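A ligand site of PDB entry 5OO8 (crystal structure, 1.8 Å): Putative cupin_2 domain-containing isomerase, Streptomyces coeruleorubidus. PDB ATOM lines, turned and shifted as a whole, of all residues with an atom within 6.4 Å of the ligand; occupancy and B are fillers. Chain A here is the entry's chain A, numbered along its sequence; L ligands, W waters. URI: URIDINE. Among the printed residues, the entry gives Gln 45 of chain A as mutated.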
ATOM      1  N   PHE A  17      33.423   5.107  -8.599  1.00  0.00           N
ATOM      2  CA  PHE A  17      32.146   4.688  -9.168  1.00  0.00           C
ATOM      3  C   PHE A  17      31.692   5.652 -10.255  1.00  0.00           C
ATOM      4  O   PHE A  17      32.203   6.770 -10.354  1.00  0.00           O
ATOM      5  CB  PHE A  17      31.081   4.605  -8.076  1.00  0.00           C
ATOM      6  CG  PHE A  17      30.871   5.894  -7.319  1.00  0.00           C
ATOM      7  CD1 PHE A  17      31.714   6.229  -6.267  1.00  0.00           C
ATOM      8  CD2 PHE A  17      29.842   6.753  -7.657  1.00  0.00           C
ATOM      9  CE1 PHE A  17      31.525   7.418  -5.565  1.00  0.00           C
ATOM     10  CE2 PHE A  17      29.654   7.942  -6.956  1.00  0.00           C
ATOM     11  CZ  PHE A  17      30.494   8.273  -5.916  1.00  0.00           C
ATOM     12  N   LYS A  19      28.536   7.794 -11.944  1.00  0.00           N
ATOM     13  CA  LYS A  19      27.290   8.440 -11.590  1.00  0.00           C
ATOM     14  C   LYS A  19      26.885   9.393 -12.716  1.00  0.00           C
ATOM     15  O   LYS A  19      27.596  10.343 -12.990  1.00  0.00           O
ATOM     16  CB  LYS A  19      27.449   9.205 -10.284  1.00  0.00           C
ATOM     17  CG  LYS A  19      26.193   9.939  -9.875  1.00  0.00           C
ATOM     18  CD  LYS A  19      26.019  10.077  -8.371  1.00  0.00           C
ATOM     19  CE  LYS A  19      26.665  11.341  -7.824  1.00  0.00           C
ATOM     20  NZ  LYS A  19      25.957  11.830  -6.615  1.00  0.00           N
ATOM     21  N   HIS A  20      25.746   9.121 -13.364  1.00  0.00           N
ATOM     22  CA  HIS A  20      25.170  10.030 -14.378  1.00  0.00           C
ATOM     23  C   HIS A  20      26.118  10.330 -15.535  1.00  0.00           C
ATOM     24  O   HIS A  20      26.046  11.409 -16.117  1.00  0.00           O
ATOM     25  CB  HIS A  20      24.719  11.358 -13.739  1.00  0.00           C
ATOM     26  CG  HIS A  20      23.860  11.199 -12.523  1.00  0.00           C
ATOM     27  ND1 HIS A  20      22.756  10.374 -12.498  1.00  0.00           N
ATOM     28  CD2 HIS A  20      23.931  11.779 -11.306  1.00  0.00           C
ATOM     29  CE1 HIS A  20      22.199  10.432 -11.295  1.00  0.00           C
ATOM     30  NE2 HIS A  20      22.881  11.290 -10.559  1.00  0.00           N
ATOM     31  N   ILE A  22      29.566  10.340 -15.307  1.00  0.00           N
ATOM     32  CA  ILE A  22      30.900  10.723 -14.838  1.00  0.00           C
ATOM     33  C   ILE A  22      31.502   9.627 -13.965  1.00  0.00           C
ATOM     34  O   ILE A  22      30.784   8.865 -13.317  1.00  0.00           O
ATOM     35  CB  ILE A  22      30.912  12.078 -14.091  1.00  0.00           C
ATOM     36  CG1 ILE A  22      30.186  12.007 -12.747  1.00  0.00           C
ATOM     37  CG2 ILE A  22      30.294  13.168 -14.959  1.00  0.00           C
ATOM     38  CD1 ILE A  22      30.514  13.165 -11.822  1.00  0.00           C
ATOM     39  N   LEU A  24      33.803   9.084 -10.754  1.00  0.00           N
ATOM     40  CA  LEU A  24      34.245   9.777  -9.545  1.00  0.00           C
ATOM     41  C   LEU A  24      35.286   8.972  -8.783  1.00  0.00           C
ATOM     42  O   LEU A  24      35.209   7.746  -8.713  1.00  0.00           O
ATOM     43  CB  LEU A  24      33.051  10.018  -8.629  1.00  0.00           C
ATOM     44  CG  LEU A  24      32.156  11.199  -9.014  1.00  0.00           C
ATOM     45  CD1 LEU A  24      30.753  11.007  -8.478  1.00  0.00           C
ATOM     46  CD2 LEU A  24      32.767  12.491  -8.492  1.00  0.00           C
ATOM     47  N   VAL A  26      36.311   9.281  -4.946  1.00  0.00           N
ATOM     48  CA  VAL A  26      36.044   9.890  -3.649  1.00  0.00           C
ATOM     49  C   VAL A  26      37.038   9.303  -2.644  1.00  0.00           C
ATOM     50  O   VAL A  26      36.935   8.138  -2.258  1.00  0.00           O
ATOM     51  CB  VAL A  26      34.601   9.640  -3.190  1.00  0.00           C
ATOM     52  CG1 VAL A  26      34.330  10.292  -1.838  1.00  0.00           C
ATOM     53  CG2 VAL A  26      33.607  10.147  -4.235  1.00  0.00           C
ATOM     54  N   THR A  35      35.405  18.931   0.702  1.00  0.00           N
ATOM     55  CA  THR A  35      35.605  17.614   0.120  1.00  0.00           C
ATOM     56  C   THR A  35      36.226  17.817  -1.253  1.00  0.00           C
ATOM     57  O   THR A  35      35.695  18.582  -2.065  1.00  0.00           O
ATOM     58  CB  THR A  35      34.239  16.908  -0.103  1.00  0.00           C
ATOM     59  OG1 THR A  35      33.487  16.922   1.118  1.00  0.00           O
ATOM     60  CG2 THR A  35      34.424  15.474  -0.601  1.00  0.00           C
ATOM     61  N   VAL A  37      37.469  15.775  -4.691  1.00  0.00           N
ATOM     62  CA  VAL A  37      37.346  14.522  -5.432  1.00  0.00           C
ATOM     63  C   VAL A  37      37.858  14.698  -6.853  1.00  0.00           C
ATOM     64  O   VAL A  37      37.999  15.817  -7.348  1.00  0.00           O
ATOM     65  CB  VAL A  37      35.879  14.020  -5.494  1.00  0.00           C
ATOM     66  CG1 VAL A  37      35.321  13.812  -4.089  1.00  0.00           C
ATOM     67  CG2 VAL A  37      34.979  14.971  -6.282  1.00  0.00           C
ATOM     68  N   VAL A  39      37.152  13.882 -10.896  1.00  0.00           N
ATOM     69  CA  VAL A  39      36.084  13.614 -11.848  1.00  0.00           C
ATOM     70  C   VAL A  39      36.707  13.365 -13.215  1.00  0.00           C
ATOM     71  O   VAL A  39      37.535  14.151 -13.682  1.00  0.00           O
ATOM     72  CB  VAL A  39      35.094  14.797 -11.949  1.00  0.00           C
ATOM     73  CG1 VAL A  39      33.961  14.475 -12.920  1.00  0.00           C
ATOM     74  CG2 VAL A  39      34.532  15.135 -10.583  1.00  0.00           C
ATOM     75  N   GLN A  45      27.974  14.960 -17.653  1.00  0.00           N
ATOM     76  CA  GLN A  45      27.115  14.591 -16.533  1.00  0.00           C
ATOM     77  C   GLN A  45      25.681  14.817 -16.993  1.00  0.00           C
ATOM     78  O   GLN A  45      25.243  15.963 -17.155  1.00  0.00           O
ATOM     79  CB  GLN A  45      27.404  15.429 -15.277  1.00  0.00           C
ATOM     80  CG  GLN A  45      26.277  15.357 -14.258  1.00  0.00           C
ATOM     81  CD  GLN A  45      26.750  15.457 -12.815  1.00  0.00           C
ATOM     82  OE1 GLN A  45      25.974  15.267 -11.879  1.00  0.00           O
ATOM     83  NE2 GLN A  45      28.036  15.746 -12.633  1.00  0.00           N
ATOM     84  N   GLN A  47      22.735  14.730 -15.753  1.00  0.00           N
ATOM     85  CA  GLN A  47      21.813  14.982 -14.669  1.00  0.00           C
ATOM     86  C   GLN A  47      22.091  16.402 -14.226  1.00  0.00           C
ATOM     87  O   GLN A  47      23.258  16.809 -14.141  1.00  0.00           O
ATOM     88  CB  GLN A  47      22.049  13.996 -13.513  1.00  0.00           C
ATOM     89  CG  GLN A  47      21.056  14.146 -12.352  1.00  0.00           C
ATOM     90  CD  GLN A  47      21.688  14.636 -11.048  1.00  0.00           C
ATOM     91  OE1 GLN A  47      22.894  14.899 -10.961  1.00  0.00           O
ATOM     92  NE2 GLN A  47      20.862  14.739 -10.011  1.00  0.00           N
ATOM     93  N   PHE A  49      21.472  19.202 -11.225  1.00  0.00           N
ATOM     94  CA  PHE A  49      21.189  19.309  -9.807  1.00  0.00           C
ATOM     95  C   PHE A  49      21.603  20.684  -9.328  1.00  0.00           C
ATOM     96  O   PHE A  49      22.297  21.408 -10.026  1.00  0.00           O
ATOM     97  CB  PHE A  49      21.970  18.248  -9.036  1.00  0.00           C
ATOM     98  CG  PHE A  49      23.450  18.482  -9.021  1.00  0.00           C
ATOM     99  CD1 PHE A  49      24.268  17.953 -10.020  1.00  0.00           C
ATOM    100  CD2 PHE A  49      24.040  19.268  -8.028  1.00  0.00           C
ATOM    101  CE1 PHE A  49      25.637  18.195 -10.018  1.00  0.00           C
ATOM    102  CE2 PHE A  49      25.409  19.510  -8.027  1.00  0.00           C
ATOM    103  CZ  PHE A  49      26.212  18.974  -9.019  1.00  0.00           C
ATOM    104  N   TYR A  56      30.592  24.401  -5.640  1.00  0.00           N
ATOM    105  CA  TYR A  56      31.280  23.347  -6.390  1.00  0.00           C
ATOM    106  C   TYR A  56      32.289  24.037  -7.299  1.00  0.00           C
ATOM    107  O   TYR A  56      31.907  24.812  -8.182  1.00  0.00           O
ATOM    108  CB  TYR A  56      30.301  22.542  -7.249  1.00  0.00           C
ATOM    109  CG  TYR A  56      29.449  21.530  -6.510  1.00  0.00           C
ATOM    110  CD1 TYR A  56      28.816  21.844  -5.311  1.00  0.00           C
ATOM    111  CD2 TYR A  56      29.238  20.264  -7.033  1.00  0.00           C
ATOM    112  CE1 TYR A  56      28.017  20.922  -4.656  1.00  0.00           C
ATOM    113  CE2 TYR A  56      28.435  19.328  -6.387  1.00  0.00           C
ATOM    114  CZ  TYR A  56      27.819  19.668  -5.201  1.00  0.00           C
ATOM    115  OH  TYR A  56      27.017  18.759  -4.541  1.00  0.00           O
ATOM    116  N   TYR A  58      35.318  23.461  -9.949  1.00  0.00           N
ATOM    117  CA  TYR A  58      35.932  22.515 -10.864  1.00  0.00           C
ATOM    118  C   TYR A  58      37.204  23.101 -11.455  1.00  0.00           C
ATOM    119  O   TYR A  58      37.173  24.121 -12.149  1.00  0.00           O
ATOM    120  CB  TYR A  58      34.964  22.183 -12.003  1.00  0.00           C
ATOM    121  CG  TYR A  58      33.651  21.560 -11.605  1.00  0.00           C
ATOM    122  CD1 TYR A  58      32.581  22.349 -11.161  1.00  0.00           C
ATOM    123  CD2 TYR A  58      33.451  20.186 -11.707  1.00  0.00           C
ATOM    124  CE1 TYR A  58      31.365  21.789 -10.817  1.00  0.00           C
ATOM    125  CE2 TYR A  58      32.233  19.608 -11.356  1.00  0.00           C
ATOM    126  CZ  TYR A  58      31.195  20.415 -10.910  1.00  0.00           C
ATOM    127  OH  TYR A  58      29.971  19.854 -10.572  1.00  0.00           O
ATOM    128  N   ILE A  90      23.381  22.892 -12.153  1.00  0.00           N
ATOM    129  CA  ILE A  90      24.606  22.463 -12.817  1.00  0.00           C
ATOM    130  C   ILE A  90      24.360  21.209 -13.628  1.00  0.00           C
ATOM    131  O   ILE A  90      23.884  20.212 -13.094  1.00  0.00           O
ATOM    132  CB  ILE A  90      25.704  22.071 -11.807  1.00  0.00           C
ATOM    133  CG1 ILE A  90      26.047  23.222 -10.868  1.00  0.00           C
ATOM    134  CG2 ILE A  90      26.960  21.594 -12.531  1.00  0.00           C
ATOM    135  CD1 ILE A  90      26.805  22.787  -9.629  1.00  0.00           C
ATOM    136  N   TYR A  92      26.853  19.493 -17.250  1.00  0.00           N
ATOM    137  CA  TYR A  92      27.938  19.792 -18.170  1.00  0.00           C
ATOM    138  C   TYR A  92      28.174  18.689 -19.192  1.00  0.00           C
ATOM    139  O   TYR A  92      27.838  17.524 -18.964  1.00  0.00           O
ATOM    140  CB  TYR A  92      29.230  20.118 -17.417  1.00  0.00           C
ATOM    141  CG  TYR A  92      29.649  19.115 -16.362  1.00  0.00           C
ATOM    142  CD1 TYR A  92      29.213  19.236 -15.042  1.00  0.00           C
ATOM    143  CD2 TYR A  92      30.505  18.077 -16.681  1.00  0.00           C
ATOM    144  CE1 TYR A  92      29.618  18.318 -14.076  1.00  0.00           C
ATOM    145  CE2 TYR A  92      30.907  17.155 -15.727  1.00  0.00           C
ATOM    146  CZ  TYR A  92      30.478  17.291 -14.422  1.00  0.00           C
ATOM    147  OH  TYR A  92      30.871  16.368 -13.474  1.00  0.00           O
ATOM    148  N   MET A  98      39.065  16.458 -14.178  1.00  0.00           N
ATOM    149  CA  MET A  98      38.857  17.595 -13.284  1.00  0.00           C
ATOM    150  C   MET A  98      39.141  17.236 -11.831  1.00  0.00           C
ATOM    151  O   MET A  98      39.053  16.064 -11.431  1.00  0.00           O
ATOM    152  CB  MET A  98      37.418  18.118 -13.394  1.00  0.00           C
ATOM    153  CG  MET A  98      36.994  18.502 -14.798  1.00  0.00           C
ATOM    154  SD  MET A  98      35.348  19.223 -14.881  1.00  0.00           S
ATOM    155  CE  MET A  98      34.319  17.812 -14.503  1.00  0.00           C
ATOM    156  N   LEU A 100      37.459  18.423  -8.343  1.00  0.00           N
ATOM    157  CA  LEU A 100      36.281  19.115  -7.822  1.00  0.00           C
ATOM    158  C   LEU A 100      36.387  19.331  -6.307  1.00  0.00           C
ATOM    159  O   LEU A 100      36.627  18.396  -5.548  1.00  0.00           O
ATOM    160  CB  LEU A 100      35.013  18.312  -8.126  1.00  0.00           C
ATOM    161  CG  LEU A 100      33.723  18.712  -7.389  1.00  0.00           C
ATOM    162  CD1 LEU A 100      33.292  20.134  -7.728  1.00  0.00           C
ATOM    163  CD2 LEU A 100      32.611  17.732  -7.738  1.00  0.00           C
ATOM    164  N   VAL A 102      34.124  20.629  -3.162  1.00  0.00           N
ATOM    165  CA  VAL A 102      32.808  20.941  -2.634  1.00  0.00           C
ATOM    166  C   VAL A 102      33.028  21.518  -1.237  1.00  0.00           C
ATOM    167  O   VAL A 102      33.596  20.855  -0.370  1.00  0.00           O
ATOM    168  CB  VAL A 102      31.913  19.682  -2.575  1.00  0.00           C
ATOM    169  CG1 VAL A 102      30.538  20.021  -1.996  1.00  0.00           C
ATOM    170  CG2 VAL A 102      31.748  19.071  -3.958  1.00  0.00           C
ATOM    171  N   PHE A 106      30.911  17.968   1.247  1.00  0.00           N
ATOM    172  CA  PHE A 106      29.811  17.384   0.500  1.00  0.00           C
ATOM    173  C   PHE A 106      28.878  16.569   1.390  1.00  0.00           C
ATOM    174  O   PHE A 106      29.335  15.722   2.164  1.00  0.00           O
ATOM    175  CB  PHE A 106      30.339  16.494  -0.630  1.00  0.00           C
ATOM    176  CG  PHE A 106      29.268  15.746  -1.372  1.00  0.00           C
ATOM    177  CD1 PHE A 106      28.502  16.376  -2.332  1.00  0.00           C
ATOM    178  CD2 PHE A 106      29.016  14.405  -1.095  1.00  0.00           C
ATOM    179  CE1 PHE A 106      27.503  15.685  -3.012  1.00  0.00           C
ATOM    180  CE2 PHE A 106      28.032  13.713  -1.778  1.00  0.00           C
ATOM    181  CZ  PHE A 106      27.270  14.356  -2.729  1.00  0.00           C
ATOM    182  N   GLU A 111      21.827  18.030  -1.905  1.00  0.00           N
ATOM    183  CA  GLU A 111      21.629  18.053  -3.336  1.00  0.00           C
ATOM    184  C   GLU A 111      20.155  17.909  -3.701  1.00  0.00           C
ATOM    185  O   GLU A 111      19.417  17.141  -3.077  1.00  0.00           O
ATOM    186  CB  GLU A 111      22.445  16.956  -4.017  1.00  0.00           C
ATOM    187  CG  GLU A 111      23.253  17.503  -5.165  1.00  0.00           C
ATOM    188  CD  GLU A 111      24.183  16.497  -5.798  1.00  0.00           C
ATOM    189  OE1 GLU A 111      23.687  15.529  -6.395  1.00  0.00           O
ATOM    190  OE2 GLU A 111      25.425  16.688  -5.717  1.00  0.00           O
HETATM  191  N1  URI L   1      29.917  13.983  -5.981  1.00  0.00           N
HETATM  192  C2  URI L   1      29.715  12.854  -5.198  1.00  0.00           C
HETATM  193  N3  URI L   1      30.467  12.809  -4.042  1.00  0.00           N
HETATM  194  C4  URI L   1      31.377  13.759  -3.610  1.00  0.00           C
HETATM  195  C5  URI L   1      31.516  14.900  -4.466  1.00  0.00           C
HETATM  196  C6  URI L   1      30.804  14.973  -5.596  1.00  0.00           C
HETATM  197  O2  URI L   1      28.939  11.954  -5.512  1.00  0.00           O
HETATM  198  O4  URI L   1      31.977  13.578  -2.545  1.00  0.00           O
HETATM  199  C1' URI L   1      29.142  14.104  -7.228  1.00  0.00           C
HETATM  200  C2' URI L   1      27.997  15.109  -7.143  1.00  0.00           C
HETATM  201  C3' URI L   1      27.796  15.461  -8.613  1.00  0.00           C
HETATM  202  C4' URI L   1      29.201  15.330  -9.204  1.00  0.00           C
HETATM  203  O2' URI L   1      26.851  14.525  -6.507  1.00  0.00           O
HETATM  204  O3' URI L   1      26.926  14.554  -9.286  1.00  0.00           O
HETATM  205  O4' URI L   1      30.000  14.601  -8.240  1.00  0.00           O
HETATM  206  C5' URI L   1      29.909  16.625  -9.538  1.00  0.00           C
HETATM  207  O5' URI L   1      29.454  17.172 -10.754  1.00  0.00           O
HETATM  208  O   HOH W   1      26.758   9.734  -4.579  1.00  0.00           O
HETATM  209  O   HOH W   2      30.096  10.437  -2.506  1.00  0.00           O
HETATM  210  O   HOH W   3      32.291  12.588  -0.036  1.00  0.00           O
HETATM  211  O   HOH W   4      24.368  14.457  -8.646  1.00  0.00           O
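O2' of the ligand is in hydrogen-bond range of NZ of Lys 19, 2.8 Å away.
The side-chain hydroxyl (OH) of Tyr 92 is in hydrogen-bond range of an oxygen (O5') of the ligand, at 3.2 Å.
An oxygen (O2') of the ligand sits at hydrogen-bond distance from the side-chain carboxylate (OE2) of Glu 111 (2.7 Å).
NE2 of Gln 45 is in hydrogen-bond range of O5' of the ligand, at 2.8 Å.
The side-chain hydroxyl of Tyr 58 is in hydrogen-bond range of an oxygen (O5') of the ligand (2.7 Å).
OG1 of Thr 35 lies within hydrogen-bond range of N of Phe 106 (2.8 Å).
O of Phe 17 sits at hydrogen-bond distance from N of Leu 24.
The backbone carbonyl oxygen of Phe 49 is in hydrogen-bond range of the backbone NH of Ile 90 (2.8 Å).
The backbone NH (N) of Gln 45 is in hydrogen-bond range of the backbone carbonyl oxygen (O) of Tyr 92 (2.9 Å).
O of Val 37 is in hydrogen-bond range of N of Leu 100 (2.8 Å).
The backbone carbonyl oxygen of Thr 35 lies within hydrogen-bond range of the backbone NH of Val 102 (2.8 Å).
OH of Tyr 56 sits at hydrogen-bond distance from OE2 of Glu 111 (2.9 Å).
The side-chain amide oxygen of Gln 45 sits close to the side-chain amide oxygen of Gln 47 (3.2 Å).
CD1 of Ile 22 touches C4' of the ligand, at 3.6 Å.
Leu 24 touches the ligand.
Thr 35 touches the ligand.
Val 37 touches the ligand.
CE1 of Phe 49 touches C3' of the ligand, at 3.8 Å.
Leu 100 touches the ligand (CD2 to C5', 3.4 Å).
CD2 of Phe 106 touches O4 of the ligand (3.4 Å).
Of the 21 residues printed, 12 come within 4 Å of the ligand.
Water W4 lies within hydrogen-bond range of OE1 of Glu 111 (2.6 Å), O3' of the ligand (2.6 Å) and OE1 of Gln 47 (2.8 Å).
Water W1 bridges NZ of Lys 19 (3.0 Å) and O2 of the ligand (3.2 Å).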
